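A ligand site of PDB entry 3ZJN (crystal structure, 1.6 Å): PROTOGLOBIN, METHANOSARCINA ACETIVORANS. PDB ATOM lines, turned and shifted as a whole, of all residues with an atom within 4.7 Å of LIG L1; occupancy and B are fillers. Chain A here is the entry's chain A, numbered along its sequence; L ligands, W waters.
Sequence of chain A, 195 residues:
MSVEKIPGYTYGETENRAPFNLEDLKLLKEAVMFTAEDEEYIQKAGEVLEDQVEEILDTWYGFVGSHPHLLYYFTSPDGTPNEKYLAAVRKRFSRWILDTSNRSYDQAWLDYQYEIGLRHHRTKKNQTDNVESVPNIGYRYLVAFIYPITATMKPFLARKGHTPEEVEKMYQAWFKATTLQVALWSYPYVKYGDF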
ATOM      1  N   TYR A   9      26.469   8.309  -5.218  1.00  0.00           N
ATOM      2  CA  TYR A   9      27.635   8.375  -6.109  1.00  0.00           C
ATOM      3  C   TYR A   9      28.551   9.531  -5.724  1.00  0.00           C
ATOM      4  O   TYR A   9      28.158  10.709  -5.835  1.00  0.00           O
ATOM      5  CB  TYR A   9      27.114   8.515  -7.549  1.00  0.00           C
ATOM      6  CG  TYR A   9      28.161   8.633  -8.605  1.00  0.00           C
ATOM      7  CD1 TYR A   9      28.881   7.521  -9.035  1.00  0.00           C
ATOM      8  CD2 TYR A   9      28.398   9.878  -9.236  1.00  0.00           C
ATOM      9  CE1 TYR A   9      29.826   7.630 -10.013  1.00  0.00           C
ATOM     10  CE2 TYR A   9      29.333  10.008 -10.233  1.00  0.00           C
ATOM     11  CZ  TYR A   9      30.044   8.879 -10.632  1.00  0.00           C
ATOM     12  OH  TYR A   9      30.982   8.968 -11.628  1.00  0.00           O
ATOM     13  N   VAL A  64      22.003 -11.721 -11.956  1.00  0.00           N
ATOM     14  CA  VAL A  64      22.166 -11.757 -10.492  1.00  0.00           C
ATOM     15  C   VAL A  64      20.885 -12.366  -9.840  1.00  0.00           C
ATOM     16  O   VAL A  64      20.964 -13.211  -8.906  1.00  0.00           O
ATOM     17  CB  VAL A  64      22.460 -10.371  -9.880  1.00  0.00           C
ATOM     18  CG1 VAL A  64      22.429 -10.452  -8.352  1.00  0.00           C
ATOM     19  CG2 VAL A  64      23.832  -9.898 -10.320  1.00  0.00           C
ATOM     20  N   LEU A  70      23.351 -15.399  -5.371  1.00  0.00           N
ATOM     21  CA  LEU A  70      23.858 -14.091  -5.856  1.00  0.00           C
ATOM     22  C   LEU A  70      22.883 -12.988  -5.465  1.00  0.00           C
ATOM     23  O   LEU A  70      23.282 -11.995  -4.849  1.00  0.00           O
ATOM     24  CB  LEU A  70      24.045 -14.107  -7.386  1.00  0.00           C
ATOM     25  CG  LEU A  70      24.943 -15.282  -7.854  1.00  0.00           C
ATOM     26  CD1 LEU A  70      25.160 -15.201  -9.371  1.00  0.00           C
ATOM     27  CD2 LEU A  70      26.279 -15.273  -7.088  1.00  0.00           C
ATOM     28  N   TYR A  73      22.914 -11.099  -1.946  1.00  0.00           N
ATOM     29  CA  TYR A  73      23.713  -9.960  -1.500  1.00  0.00           C
ATOM     30  C   TYR A  73      22.900  -8.704  -1.495  1.00  0.00           C
ATOM     31  O   TYR A  73      23.354  -7.712  -0.918  1.00  0.00           O
ATOM     32  CB  TYR A  73      25.009  -9.823  -2.364  1.00  0.00           C
ATOM     33  CG  TYR A  73      25.867 -10.998  -2.045  1.00  0.00           C
ATOM     34  CD1 TYR A  73      26.448 -11.126  -0.758  1.00  0.00           C
ATOM     35  CD2 TYR A  73      25.994 -12.085  -2.937  1.00  0.00           C
ATOM     36  CE1 TYR A  73      27.175 -12.265  -0.397  1.00  0.00           C
ATOM     37  CE2 TYR A  73      26.718 -13.184  -2.577  1.00  0.00           C
ATOM     38  CZ  TYR A  73      27.291 -13.272  -1.320  1.00  0.00           C
ATOM     39  OH  TYR A  73      27.989 -14.416  -0.945  1.00  0.00           O
ATOM     40  N   PHE A  74      21.710  -8.738  -2.090  1.00  0.00           N
ATOM     41  CA  PHE A  74      20.780  -7.596  -2.113  1.00  0.00           C
ATOM     42  C   PHE A  74      19.598  -7.789  -1.175  1.00  0.00           C
ATOM     43  O   PHE A  74      18.723  -6.922  -1.057  1.00  0.00           O
ATOM     44  CB  PHE A  74      20.238  -7.350  -3.542  1.00  0.00           C
ATOM     45  CG  PHE A  74      21.222  -6.675  -4.462  1.00  0.00           C
ATOM     46  CD1 PHE A  74      21.378  -5.257  -4.426  1.00  0.00           C
ATOM     47  CD2 PHE A  74      21.995  -7.426  -5.357  1.00  0.00           C
ATOM     48  CE1 PHE A  74      22.275  -4.595  -5.291  1.00  0.00           C
ATOM     49  CE2 PHE A  74      22.900  -6.776  -6.222  1.00  0.00           C
ATOM     50  CZ  PHE A  74      23.053  -5.336  -6.167  1.00  0.00           C
ATOM     51  N   TYR A  85      17.210  -1.047  -2.326  1.00  0.00           N
ATOM     52  CA  TYR A  85      18.658  -1.258  -2.425  1.00  0.00           C
ATOM     53  C   TYR A  85      19.050  -1.528  -3.869  1.00  0.00           C
ATOM     54  O   TYR A  85      19.961  -0.859  -4.392  1.00  0.00           O
ATOM     55  CB  TYR A  85      19.016  -2.438  -1.557  1.00  0.00           C
ATOM     56  CG  TYR A  85      20.462  -2.741  -1.298  1.00  0.00           C
ATOM     57  CD1 TYR A  85      21.452  -1.764  -1.345  1.00  0.00           C
ATOM     58  CD2 TYR A  85      20.820  -4.029  -0.894  1.00  0.00           C
ATOM     59  CE1 TYR A  85      22.777  -2.085  -1.055  1.00  0.00           C
ATOM     60  CE2 TYR A  85      22.156  -4.361  -0.585  1.00  0.00           C
ATOM     61  CZ  TYR A  85      23.120  -3.391  -0.658  1.00  0.00           C
ATOM     62  OH  TYR A  85      24.432  -3.707  -0.326  1.00  0.00           O
ATOM     63  N   VAL A  89      21.369   0.982  -6.225  1.00  0.00           N
ATOM     64  CA  VAL A  89      22.616   0.464  -6.788  1.00  0.00           C
ATOM     65  C   VAL A  89      22.618   0.481  -8.289  1.00  0.00           C
ATOM     66  O   VAL A  89      23.646   0.799  -8.912  1.00  0.00           O
ATOM     67  CB  VAL A  89      22.971  -0.919  -6.290  1.00  0.00           C
ATOM     68  CG1 VAL A  89      24.234  -1.379  -7.020  1.00  0.00           C
ATOM     69  CG2 VAL A  89      23.199  -0.882  -4.757  1.00  0.00           C
ATOM     70  N   ARG A  92      23.930   3.636  -9.809  1.00  0.00           N
ATOM     71  CA  ARG A  92      25.381   3.749  -9.735  1.00  0.00           C
ATOM     72  C   ARG A  92      26.083   2.764 -10.683  1.00  0.00           C
ATOM     73  O   ARG A  92      27.169   3.037 -11.212  1.00  0.00           O
ATOM     74  CB  ARG A  92      25.819   3.584  -8.271  1.00  0.00           C
ATOM     75  CG  ARG A  92      25.220   4.723  -7.365  1.00  0.00           C
ATOM     76  CD  ARG A  92      25.956   4.957  -6.032  1.00  0.00           C
ATOM     77  NE  ARG A  92      25.875   3.759  -5.184  1.00  0.00           N
ATOM     78  CZ  ARG A  92      24.852   3.480  -4.381  1.00  0.00           C
ATOM     79  NH1 ARG A  92      23.818   4.300  -4.306  1.00  0.00           N
ATOM     80  NH2 ARG A  92      24.842   2.343  -3.677  1.00  0.00           N
ATOM     81  N   PHE A  93      25.514   1.581 -10.860  1.00  0.00           N
ATOM     82  CA  PHE A  93      26.109   0.624 -11.802  1.00  0.00           C
ATOM     83  C   PHE A  93      26.019   1.199 -13.223  1.00  0.00           C
ATOM     84  O   PHE A  93      26.995   1.206 -13.950  1.00  0.00           O
ATOM     85  CB  PHE A  93      25.403  -0.713 -11.699  1.00  0.00           C
ATOM     86  CG  PHE A  93      26.039  -1.814 -12.542  1.00  0.00           C
ATOM     87  CD1 PHE A  93      25.724  -1.950 -13.926  1.00  0.00           C
ATOM     88  CD2 PHE A  93      26.891  -2.738 -11.955  1.00  0.00           C
ATOM     89  CE1 PHE A  93      26.312  -2.968 -14.713  1.00  0.00           C
ATOM     90  CE2 PHE A  93      27.468  -3.793 -12.708  1.00  0.00           C
ATOM     91  CZ  PHE A  93      27.177  -3.922 -14.076  1.00  0.00           C
ATOM     92  N   TRP A  96      28.667   3.588 -13.682  1.00  0.00           N
ATOM     93  CA  TRP A  96      29.959   2.896 -13.761  1.00  0.00           C
ATOM     94  C   TRP A  96      30.305   2.443 -15.163  1.00  0.00           C
ATOM     95  O   TRP A  96      31.465   2.456 -15.576  1.00  0.00           O
ATOM     96  CB  TRP A  96      29.964   1.721 -12.786  1.00  0.00           C
ATOM     97  CG  TRP A  96      31.120   0.803 -12.958  1.00  0.00           C
ATOM     98  CD1 TRP A  96      32.377   0.943 -12.448  1.00  0.00           C
ATOM     99  CD2 TRP A  96      31.129  -0.420 -13.726  1.00  0.00           C
ATOM    100  NE1 TRP A  96      33.152  -0.125 -12.838  1.00  0.00           N
ATOM    101  CE2 TRP A  96      32.414  -0.949 -13.647  1.00  0.00           C
ATOM    102  CE3 TRP A  96      30.179  -1.065 -14.516  1.00  0.00           C
ATOM    103  CZ2 TRP A  96      32.779  -2.163 -14.259  1.00  0.00           C
ATOM    104  CZ3 TRP A  96      30.539  -2.328 -15.106  1.00  0.00           C
ATOM    105  CH2 TRP A  96      31.816  -2.803 -15.006  1.00  0.00           C
ATOM    106  N   TYR A 112      38.073   6.192  -6.289  1.00  0.00           N
ATOM    107  CA  TYR A 112      36.721   5.666  -6.378  1.00  0.00           C
ATOM    108  C   TYR A 112      36.765   4.150  -6.463  1.00  0.00           C
ATOM    109  O   TYR A 112      35.880   3.504  -5.997  1.00  0.00           O
ATOM    110  CB  TYR A 112      35.886   6.303  -7.507  1.00  0.00           C
ATOM    111  CG  TYR A 112      34.415   6.237  -7.174  1.00  0.00           C
ATOM    112  CD1 TYR A 112      33.883   6.948  -6.073  1.00  0.00           C
ATOM    113  CD2 TYR A 112      33.538   5.469  -7.951  1.00  0.00           C
ATOM    114  CE1 TYR A 112      32.581   6.853  -5.747  1.00  0.00           C
ATOM    115  CE2 TYR A 112      32.185   5.363  -7.606  1.00  0.00           C
ATOM    116  CZ  TYR A 112      31.707   6.095  -6.515  1.00  0.00           C
ATOM    117  OH  TYR A 112      30.381   6.057  -6.146  1.00  0.00           O
ATOM    118  N   ILE A 116      34.600   1.697  -4.236  1.00  0.00           N
ATOM    119  CA  ILE A 116      33.720   0.619  -4.751  1.00  0.00           C
ATOM    120  C   ILE A 116      34.086  -0.717  -4.104  1.00  0.00           C
ATOM    121  O   ILE A 116      33.183  -1.433  -3.673  1.00  0.00           O
ATOM    122  CB  ILE A 116      33.757   0.484  -6.314  1.00  0.00           C
ATOM    123  CG1 ILE A 116      33.195   1.772  -6.969  1.00  0.00           C
ATOM    124  CG2 ILE A 116      32.896  -0.696  -6.779  1.00  0.00           C
ATOM    125  CD1 ILE A 116      33.297   1.775  -8.415  1.00  0.00           C
ATOM    126  N   ARG A 119      32.710  -0.763  -0.594  1.00  0.00           N
ATOM    127  CA  ARG A 119      31.246  -0.900  -0.595  1.00  0.00           C
ATOM    128  C   ARG A 119      30.768  -2.348  -0.871  1.00  0.00           C
ATOM    129  O   ARG A 119      29.711  -2.761  -0.393  1.00  0.00           O
ATOM    130  CB  ARG A 119      30.634   0.082  -1.608  1.00  0.00           C
ATOM    131  CG  ARG A 119      30.778   1.557  -1.136  1.00  0.00           C
ATOM    132  CD  ARG A 119      30.153   2.447  -2.195  1.00  0.00           C
ATOM    133  NE  ARG A 119      30.376   3.832  -1.835  1.00  0.00           N
ATOM    134  CZ  ARG A 119      29.795   4.884  -2.409  1.00  0.00           C
ATOM    135  NH1 ARG A 119      28.915   4.735  -3.386  1.00  0.00           N
ATOM    136  NH2 ARG A 119      30.076   6.120  -1.963  1.00  0.00           N
ATOM    137  N   HIS A 120      31.520  -3.108  -1.631  1.00  0.00           N
ATOM    138  CA  HIS A 120      31.220  -4.576  -1.732  1.00  0.00           C
ATOM    139  C   HIS A 120      31.605  -5.271  -0.458  1.00  0.00           C
ATOM    140  O   HIS A 120      30.936  -6.240  -0.017  1.00  0.00           O
ATOM    141  CB  HIS A 120      31.936  -5.203  -2.936  1.00  0.00           C
ATOM    142  CG  HIS A 120      31.325  -4.836  -4.225  1.00  0.00           C
ATOM    143  ND1 HIS A 120      31.558  -3.611  -4.856  1.00  0.00           N
ATOM    144  CD2 HIS A 120      30.424  -5.499  -5.012  1.00  0.00           C
ATOM    145  CE1 HIS A 120      30.881  -3.579  -5.983  1.00  0.00           C
ATOM    146  NE2 HIS A 120      30.164  -4.682  -6.088  1.00  0.00           N
ATOM    147  N   LYS A 124      32.135  -1.089   4.141  1.00  0.00           N
ATOM    148  CA  LYS A 124      31.151  -0.046   3.826  1.00  0.00           C
ATOM    149  C   LYS A 124      29.848  -0.580   3.212  1.00  0.00           C
ATOM    150  O   LYS A 124      28.947   0.189   2.952  1.00  0.00           O
ATOM    151  CB  LYS A 124      31.763   0.986   2.886  1.00  0.00           C
ATOM    152  CG  LYS A 124      32.842   1.845   3.537  1.00  0.00           C
ATOM    153  CD  LYS A 124      33.098   3.131   2.789  1.00  0.00           C
ATOM    154  CE  LYS A 124      31.968   4.144   2.945  1.00  0.00           C
ATOM    155  NZ  LYS A 124      32.354   5.457   2.337  1.00  0.00           N
ATOM    156  N   LYS A 125      29.738  -1.892   3.024  1.00  0.00           N
ATOM    157  CA  LYS A 125      28.482  -2.400   2.483  1.00  0.00           C
ATOM    158  C   LYS A 125      27.264  -1.962   3.328  1.00  0.00           C
ATOM    159  O   LYS A 125      27.326  -1.954   4.555  1.00  0.00           O
ATOM    160  CB  LYS A 125      28.515  -3.908   2.318  1.00  0.00           C
ATOM    161  CG  LYS A 125      27.325  -4.464   1.474  1.00  0.00           C
ATOM    162  CD  LYS A 125      27.410  -6.010   1.352  1.00  0.00           C
ATOM    163  CE  LYS A 125      26.233  -6.497   0.504  1.00  0.00           C
ATOM    164  NZ  LYS A 125      24.847  -6.281   1.058  1.00  0.00           N
ATOM    165  N   ASN A 126      26.207  -1.558   2.617  1.00  0.00           N
ATOM    166  CA  ASN A 126      24.856  -1.228   3.132  1.00  0.00           C
ATOM    167  C   ASN A 126      24.800   0.192   3.638  1.00  0.00           C
ATOM    168  O   ASN A 126      23.734   0.656   3.981  1.00  0.00           O
ATOM    169  CB  ASN A 126      24.392  -2.154   4.238  1.00  0.00           C
ATOM    170  CG  ASN A 126      24.489  -3.573   3.857  1.00  0.00           C
ATOM    171  OD1 ASN A 126      24.046  -3.916   2.743  1.00  0.00           O
ATOM    172  ND2 ASN A 126      25.093  -4.400   4.715  1.00  0.00           N
ATOM    173  N   GLN A 127      25.945   0.853   3.696  1.00  0.00           N
ATOM    174  CA  GLN A 127      26.024   2.176   4.325  1.00  0.00           C
ATOM    175  C   GLN A 127      25.598   3.272   3.379  1.00  0.00           C
ATOM    176  O   GLN A 127      24.977   4.255   3.797  1.00  0.00           O
ATOM    177  CB  GLN A 127      27.428   2.453   4.828  1.00  0.00           C
ATOM    178  CG  GLN A 127      27.794   1.774   6.156  1.00  0.00           C
ATOM    179  CD  GLN A 127      29.132   2.227   6.695  1.00  0.00           C
ATOM    180  OE1 GLN A 127      29.525   3.411   6.536  1.00  0.00           O
ATOM    181  NE2 GLN A 127      29.860   1.306   7.332  1.00  0.00           N
ATOM    182  N   THR A 128      25.939   3.132   2.112  1.00  0.00           N
ATOM    183  CA  THR A 128      25.646   4.185   1.146  1.00  0.00           C
ATOM    184  C   THR A 128      24.140   4.444   1.019  1.00  0.00           C
ATOM    185  O   THR A 128      23.676   5.605   0.930  1.00  0.00           O
ATOM    186  CB  THR A 128      26.321   3.862  -0.201  1.00  0.00           C
ATOM    187  OG1 THR A 128      27.717   3.801   0.049  1.00  0.00           O
ATOM    188  CG2 THR A 128      26.019   4.979  -1.299  1.00  0.00           C
ATOM    189  N   ILE A 137      30.034  -9.090   0.759  1.00  0.00           N
ATOM    190  CA  ILE A 137      29.981  -9.922  -0.456  1.00  0.00           C
ATOM    191  C   ILE A 137      31.249 -10.752  -0.537  1.00  0.00           C
ATOM    192  O   ILE A 137      32.368 -10.229  -0.684  1.00  0.00           O
ATOM    193  CB  ILE A 137      29.778  -9.056  -1.745  1.00  0.00           C
ATOM    194  CG1 ILE A 137      28.508  -8.213  -1.632  1.00  0.00           C
ATOM    195  CG2 ILE A 137      29.741 -10.003  -2.989  1.00  0.00           C
ATOM    196  CD1 ILE A 137      28.462  -7.044  -2.662  1.00  0.00           C
ATOM    197  N   TYR A 141      33.084 -14.223  -5.228  1.00  0.00           N
ATOM    198  CA  TYR A 141      32.134 -13.804  -6.250  1.00  0.00           C
ATOM    199  C   TYR A 141      32.544 -12.575  -7.001  1.00  0.00           C
ATOM    200  O   TYR A 141      32.160 -12.433  -8.159  1.00  0.00           O
ATOM    201  CB  TYR A 141      30.695 -13.651  -5.706  1.00  0.00           C
ATOM    202  CG  TYR A 141      30.177 -14.996  -5.178  1.00  0.00           C
ATOM    203  CD1 TYR A 141      30.028 -16.096  -6.044  1.00  0.00           C
ATOM    204  CD2 TYR A 141      29.835 -15.167  -3.830  1.00  0.00           C
ATOM    205  CE1 TYR A 141      29.577 -17.304  -5.582  1.00  0.00           C
ATOM    206  CE2 TYR A 141      29.357 -16.439  -3.330  1.00  0.00           C
ATOM    207  CZ  TYR A 141      29.224 -17.463  -4.252  1.00  0.00           C
ATOM    208  OH  TYR A 141      28.796 -18.719  -3.843  1.00  0.00           O
ATOM    209  N   LEU A 142      33.274 -11.666  -6.335  1.00  0.00           N
ATOM    210  CA  LEU A 142      33.773 -10.482  -7.058  1.00  0.00           C
ATOM    211  C   LEU A 142      34.697 -10.907  -8.211  1.00  0.00           C
ATOM    212  O   LEU A 142      34.593 -10.393  -9.323  1.00  0.00           O
ATOM    213  CB  LEU A 142      34.505  -9.517  -6.121  1.00  0.00           C
ATOM    214  CG  LEU A 142      33.738  -8.319  -5.564  1.00  0.00           C
ATOM    215  CD1 LEU A 142      32.677  -8.827  -4.616  1.00  0.00           C
ATOM    216  CD2 LEU A 142      34.672  -7.341  -4.862  1.00  0.00           C
ATOM    217  N   PHE A 145      32.741 -12.657 -10.933  1.00  0.00           N
ATOM    218  CA  PHE A 145      31.862 -11.811 -11.726  1.00  0.00           C
ATOM    219  C   PHE A 145      32.574 -11.082 -12.867  1.00  0.00           C
ATOM    220  O   PHE A 145      31.903 -10.591 -13.764  1.00  0.00           O
ATOM    221  CB  PHE A 145      31.136 -10.784 -10.847  1.00  0.00           C
ATOM    222  CG  PHE A 145      29.798 -11.239 -10.342  1.00  0.00           C
ATOM    223  CD1 PHE A 145      29.523 -12.613 -10.136  1.00  0.00           C
ATOM    224  CD2 PHE A 145      28.842 -10.304  -9.969  1.00  0.00           C
ATOM    225  CE1 PHE A 145      28.277 -13.032  -9.607  1.00  0.00           C
ATOM    226  CE2 PHE A 145      27.598 -10.665  -9.493  1.00  0.00           C
ATOM    227  CZ  PHE A 145      27.300 -12.055  -9.283  1.00  0.00           C
ATOM    228  N   ILE A 146      33.913 -11.098 -12.892  1.00  0.00           N
ATOM    229  CA  ILE A 146      34.619 -10.635 -14.094  1.00  0.00           C
ATOM    230  C   ILE A 146      34.014 -11.294 -15.356  1.00  0.00           C
ATOM    231  O   ILE A 146      33.746 -10.644 -16.354  1.00  0.00           O
ATOM    232  CB  ILE A 146      36.122 -10.908 -14.028  1.00  0.00           C
ATOM    233  CG1 ILE A 146      36.785 -10.113 -12.881  1.00  0.00           C
ATOM    234  CG2 ILE A 146      36.779 -10.559 -15.412  1.00  0.00           C
ATOM    235  CD1 ILE A 146      38.156 -10.641 -12.522  1.00  0.00           C
ATOM    236  N   ILE A 149      30.308 -10.115 -16.265  1.00  0.00           N
ATOM    237  CA  ILE A 149      30.308  -8.720 -16.741  1.00  0.00           C
ATOM    238  C   ILE A 149      30.651  -8.690 -18.247  1.00  0.00           C
ATOM    239  O   ILE A 149      29.955  -8.018 -19.055  1.00  0.00           O
ATOM    240  CB  ILE A 149      31.285  -7.815 -15.942  1.00  0.00           C
ATOM    241  CG1 ILE A 149      30.742  -7.533 -14.555  1.00  0.00           C
ATOM    242  CG2 ILE A 149      31.458  -6.461 -16.638  1.00  0.00           C
ATOM    243  CD1 ILE A 149      29.678  -6.417 -14.555  1.00  0.00           C
ATOM    244  N   THR A 178      37.748  -4.407 -16.708  1.00  0.00           N
ATOM    245  CA  THR A 178      36.943  -5.013 -15.647  1.00  0.00           C
ATOM    246  C   THR A 178      37.880  -5.830 -14.713  1.00  0.00           C
ATOM    247  O   THR A 178      37.800  -5.748 -13.486  1.00  0.00           O
ATOM    248  CB  THR A 178      35.834  -5.914 -16.242  1.00  0.00           C
ATOM    249  OG1 THR A 178      34.985  -5.095 -17.079  1.00  0.00           O
ATOM    250  CG2 THR A 178      35.013  -6.596 -15.136  1.00  0.00           C
ATOM    251  N   VAL A 182      38.513  -5.150 -10.629  1.00  0.00           N
ATOM    252  CA  VAL A 182      38.285  -6.139  -9.580  1.00  0.00           C
ATOM    253  C   VAL A 182      39.616  -6.393  -8.807  1.00  0.00           C
ATOM    254  O   VAL A 182      39.610  -6.578  -7.594  1.00  0.00           O
ATOM    255  CB  VAL A 182      37.692  -7.433 -10.176  1.00  0.00           C
ATOM    256  CG1 VAL A 182      37.736  -8.593  -9.167  1.00  0.00           C
ATOM    257  CG2 VAL A 182      36.249  -7.163 -10.638  1.00  0.00           C
ATOM    258  N   TRP A 185      39.758  -3.749  -6.351  1.00  0.00           N
ATOM    259  CA  TRP A 185      38.719  -3.943  -5.355  1.00  0.00           C
ATOM    260  C   TRP A 185      39.077  -4.982  -4.319  1.00  0.00           C
ATOM    261  O   TRP A 185      38.546  -4.961  -3.210  1.00  0.00           O
ATOM    262  CB  TRP A 185      37.346  -4.241  -5.964  1.00  0.00           C
ATOM    263  CG  TRP A 185      36.860  -3.209  -6.958  1.00  0.00           C
ATOM    264  CD1 TRP A 185      37.441  -2.007  -7.310  1.00  0.00           C
ATOM    265  CD2 TRP A 185      35.660  -3.303  -7.743  1.00  0.00           C
ATOM    266  NE1 TRP A 185      36.704  -1.386  -8.252  1.00  0.00           N
ATOM    267  CE2 TRP A 185      35.591  -2.127  -8.536  1.00  0.00           C
ATOM    268  CE3 TRP A 185      34.639  -4.263  -7.843  1.00  0.00           C
ATOM    269  CZ2 TRP A 185      34.562  -1.901  -9.449  1.00  0.00           C
ATOM    270  CZ3 TRP A 185      33.613  -4.046  -8.726  1.00  0.00           C
ATOM    271  CH2 TRP A 185      33.556  -2.872  -9.511  1.00  0.00           C
HETATM  272  C1  LIG L   1      27.599  -2.144  -5.935  1.00  0.00           C
HETATM  273  C2  LIG L   1      29.823  -3.330 -10.166  1.00  0.00           C
HETATM  274  C3  LIG L   1      30.534  -7.699  -8.201  1.00  0.00           C
HETATM  275  C4  LIG L   1      26.461  -6.855  -5.716  1.00  0.00           C
HETATM  276  C5  LIG L   1      28.223  -2.055  -7.164  1.00  0.00           C
HETATM  277  C6  LIG L   1      28.435  -0.866  -7.952  1.00  0.00           C
HETATM  278  C7  LIG L   1      29.058  -1.199  -9.099  1.00  0.00           C
HETATM  279  C8  LIG L   1      29.206  -2.638  -9.132  1.00  0.00           C
HETATM  280  C9  LIG L   1      29.517  -0.265 -10.244  1.00  0.00           C
HETATM  281  C10 LIG L   1      28.041   0.551  -7.432  1.00  0.00           C
HETATM  282  C11 LIG L   1      29.304   1.229  -6.907  1.00  0.00           C
HETATM  283  C12 LIG L   1      29.030   2.588  -6.344  1.00  0.00           C
HETATM  284  O1  LIG L   1      29.326   3.595  -7.039  1.00  0.00           O
HETATM  285  O2  LIG L   1      28.509   2.648  -5.217  1.00  0.00           O
HETATM  286  C13 LIG L   1      30.324  -4.603  -9.978  1.00  0.00           C
HETATM  287  C14 LIG L   1      31.285  -5.290 -10.794  1.00  0.00           C
HETATM  288  C15 LIG L   1      31.502  -6.525 -10.237  1.00  0.00           C
HETATM  289  C16 LIG L   1      30.632  -6.616  -9.069  1.00  0.00           C
HETATM  290  C17 LIG L   1      31.942  -4.743 -12.073  1.00  0.00           C
HETATM  291  C18 LIG L   1      32.481  -7.630 -10.659  1.00  0.00           C
HETATM  292  C19 LIG L   1      33.164  -7.689 -11.803  1.00  0.00           C
HETATM  293  C20 LIG L   1      29.410  -7.922  -7.444  1.00  0.00           C
HETATM  294  C21 LIG L   1      28.916  -9.139  -6.913  1.00  0.00           C
HETATM  295  C22 LIG L   1      27.770  -8.919  -6.286  1.00  0.00           C
HETATM  296  C23 LIG L   1      27.519  -7.476  -6.317  1.00  0.00           C
HETATM  297  C24 LIG L   1      29.574 -10.531  -7.092  1.00  0.00           C
HETATM  298  C25 LIG L   1      26.926 -10.018  -5.631  1.00  0.00           C
HETATM  299  C26 LIG L   1      25.622 -10.100  -5.984  1.00  0.00           C
HETATM  300  C27 LIG L   1      26.532  -5.526  -5.340  1.00  0.00           C
HETATM  301  C28 LIG L   1      25.912  -4.949  -4.191  1.00  0.00           C
HETATM  302  C29 LIG L   1      26.279  -3.471  -4.263  1.00  0.00           C
HETATM  303  C30 LIG L   1      27.071  -3.328  -5.460  1.00  0.00           C
HETATM  304  C31 LIG L   1      25.060  -5.658  -3.120  1.00  0.00           C
HETATM  305  C32 LIG L   1      25.957  -2.383  -3.238  1.00  0.00           C
HETATM  306  C33 LIG L   1      27.107  -2.449  -2.197  1.00  0.00           C
HETATM  307  C34 LIG L   1      26.801  -1.347  -1.216  1.00  0.00           C
HETATM  308  O3  LIG L   1      26.029  -1.587  -0.232  1.00  0.00           O
HETATM  309  O4  LIG L   1      27.246  -0.197  -1.463  1.00  0.00           O
HETATM  310  N1  LIG L   1      28.630  -3.113  -7.940  1.00  0.00           N
HETATM  311  N2  LIG L   1      29.937  -5.402  -8.919  1.00  0.00           N
HETATM  312  N3  LIG L   1      28.560  -6.923  -7.060  1.00  0.00           N
HETATM  313  N4  LIG L   1      27.221  -4.597  -6.067  1.00  0.00           N
HETATM  314 FE1  LIG L   1      28.594  -5.013  -7.515  1.00  0.00          FE
HETATM  315  C1  LG2 L   2      26.931  -5.294  -8.868  1.00  0.00           C
HETATM  316  N1  LG2 L   2      26.009  -5.304  -9.488  1.00  0.00           N
HETATM  317  O   HOH W   1      24.374   0.639   0.370  1.00  0.00           O
HETATM  318  O   HOH W   2      27.209   0.673  -3.985  1.00  0.00           O
HETATM  319  O   HOH W   3      29.515   3.850  -9.712  1.00  0.00           O
HETATM  320  O   HOH W   4      27.652   1.220   0.742  1.00  0.00           O
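FE1 of LIG L1 is bound by NE2 of His 120 (2.1 Å). An oxygen (O3) of LIG L1 sits at hydrogen-bond distance from the side-chain hydroxyl of Tyr 85. The guanidinium group (NH1) of Arg 119 lies within salt-bridge range of an oxygen (O2) of LIG L1 (2.8 Å). The side-chain hydroxyl of Tyr 112 is in hydrogen-bond range of an oxygen (O1) of LIG L1, 2.8 Å away. N of Asn 126 is in hydrogen-bond range of O3 of LIG L1, 2.9 Å away. An oxygen (O2) of LIG L1 lies within salt-bridge range of the guanidinium group (NE) of Arg 92, 2.9 Å away.
The backbone NH of Ile 137 lies within hydrogen-bond range of the backbone carbonyl oxygen of His 120, at 3.1 Å. A ring nitrogen (ND1) of His 120 is in hydrogen-bond range of the backbone carbonyl oxygen of Ile 116, 3.0 Å away. The side-chain amide oxygen (OD1) of Asn 126 is in hydrogen-bond range of the side-chain hydroxyl (OH) of Tyr 85 (3.1 Å). The side-chain amino group of Lys 125 is in hydrogen-bond range of the side-chain hydroxyl of Tyr 85 (3.0 Å). The guanidinium group of Arg 119 lies within hydrogen-bond range of the side-chain hydroxyl of Tyr 112 (3.4 Å). The guanidinium group (NE) of Arg 119 is in hydrogen-bond range of the side-chain hydroxyl (OG1) of Thr 128. OD1 of Asn 126 lies within hydrogen-bond range of NZ of Lys 125 (3.0 Å). The side-chain amino group of Lys 125 sits at hydrogen-bond distance from the backbone carbonyl oxygen of Tyr 73, 2.9 Å away.
Residues that only touch LIG L1: Val 64, Leu 70, Tyr 73, Phe 74, Val 89, Phe 93, Trp 96, Ile 116, Lys 125, Ile 137, Tyr 141, Leu 142, Phe 145, Ile 146, Ile 149, Thr 178, Val 182 and Trp 185. Hydrophobic or aromatic side chains that line LIG L1: Val 64, Tyr 73, Phe 74, Tyr 85, Val 89, Phe 93, Trp 96, Tyr 112, Ile 116, His 120, Ile 137, Tyr 141, Phe 145, Ile 149, Val 182 and Trp 185. The nearest printed residue that does not touch LIG L1 is Thr 128 (4.3 Å).
Water W4 lies within hydrogen-bond range of an oxygen (O4) of LIG L1 (2.7 Å), the side-chain hydroxyl (OG1) of Thr 128 (2.7 Å), the backbone carbonyl oxygen (O) of Lys 124 (2.8 Å) and the backbone NH (N) of Gln 127 (3.4 Å). Water W2 bridges an oxygen (O2) of LIG L1 (2.7 Å) and the guanidinium group of Arg 92 (2.9 Å). Water W3 bridges O1 of LIG L1 (2.7 Å) and O of Arg 92 (2.9 Å). Water W1 lies within hydrogen-bond range of O3 of LIG L1 and N of Thr 128.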
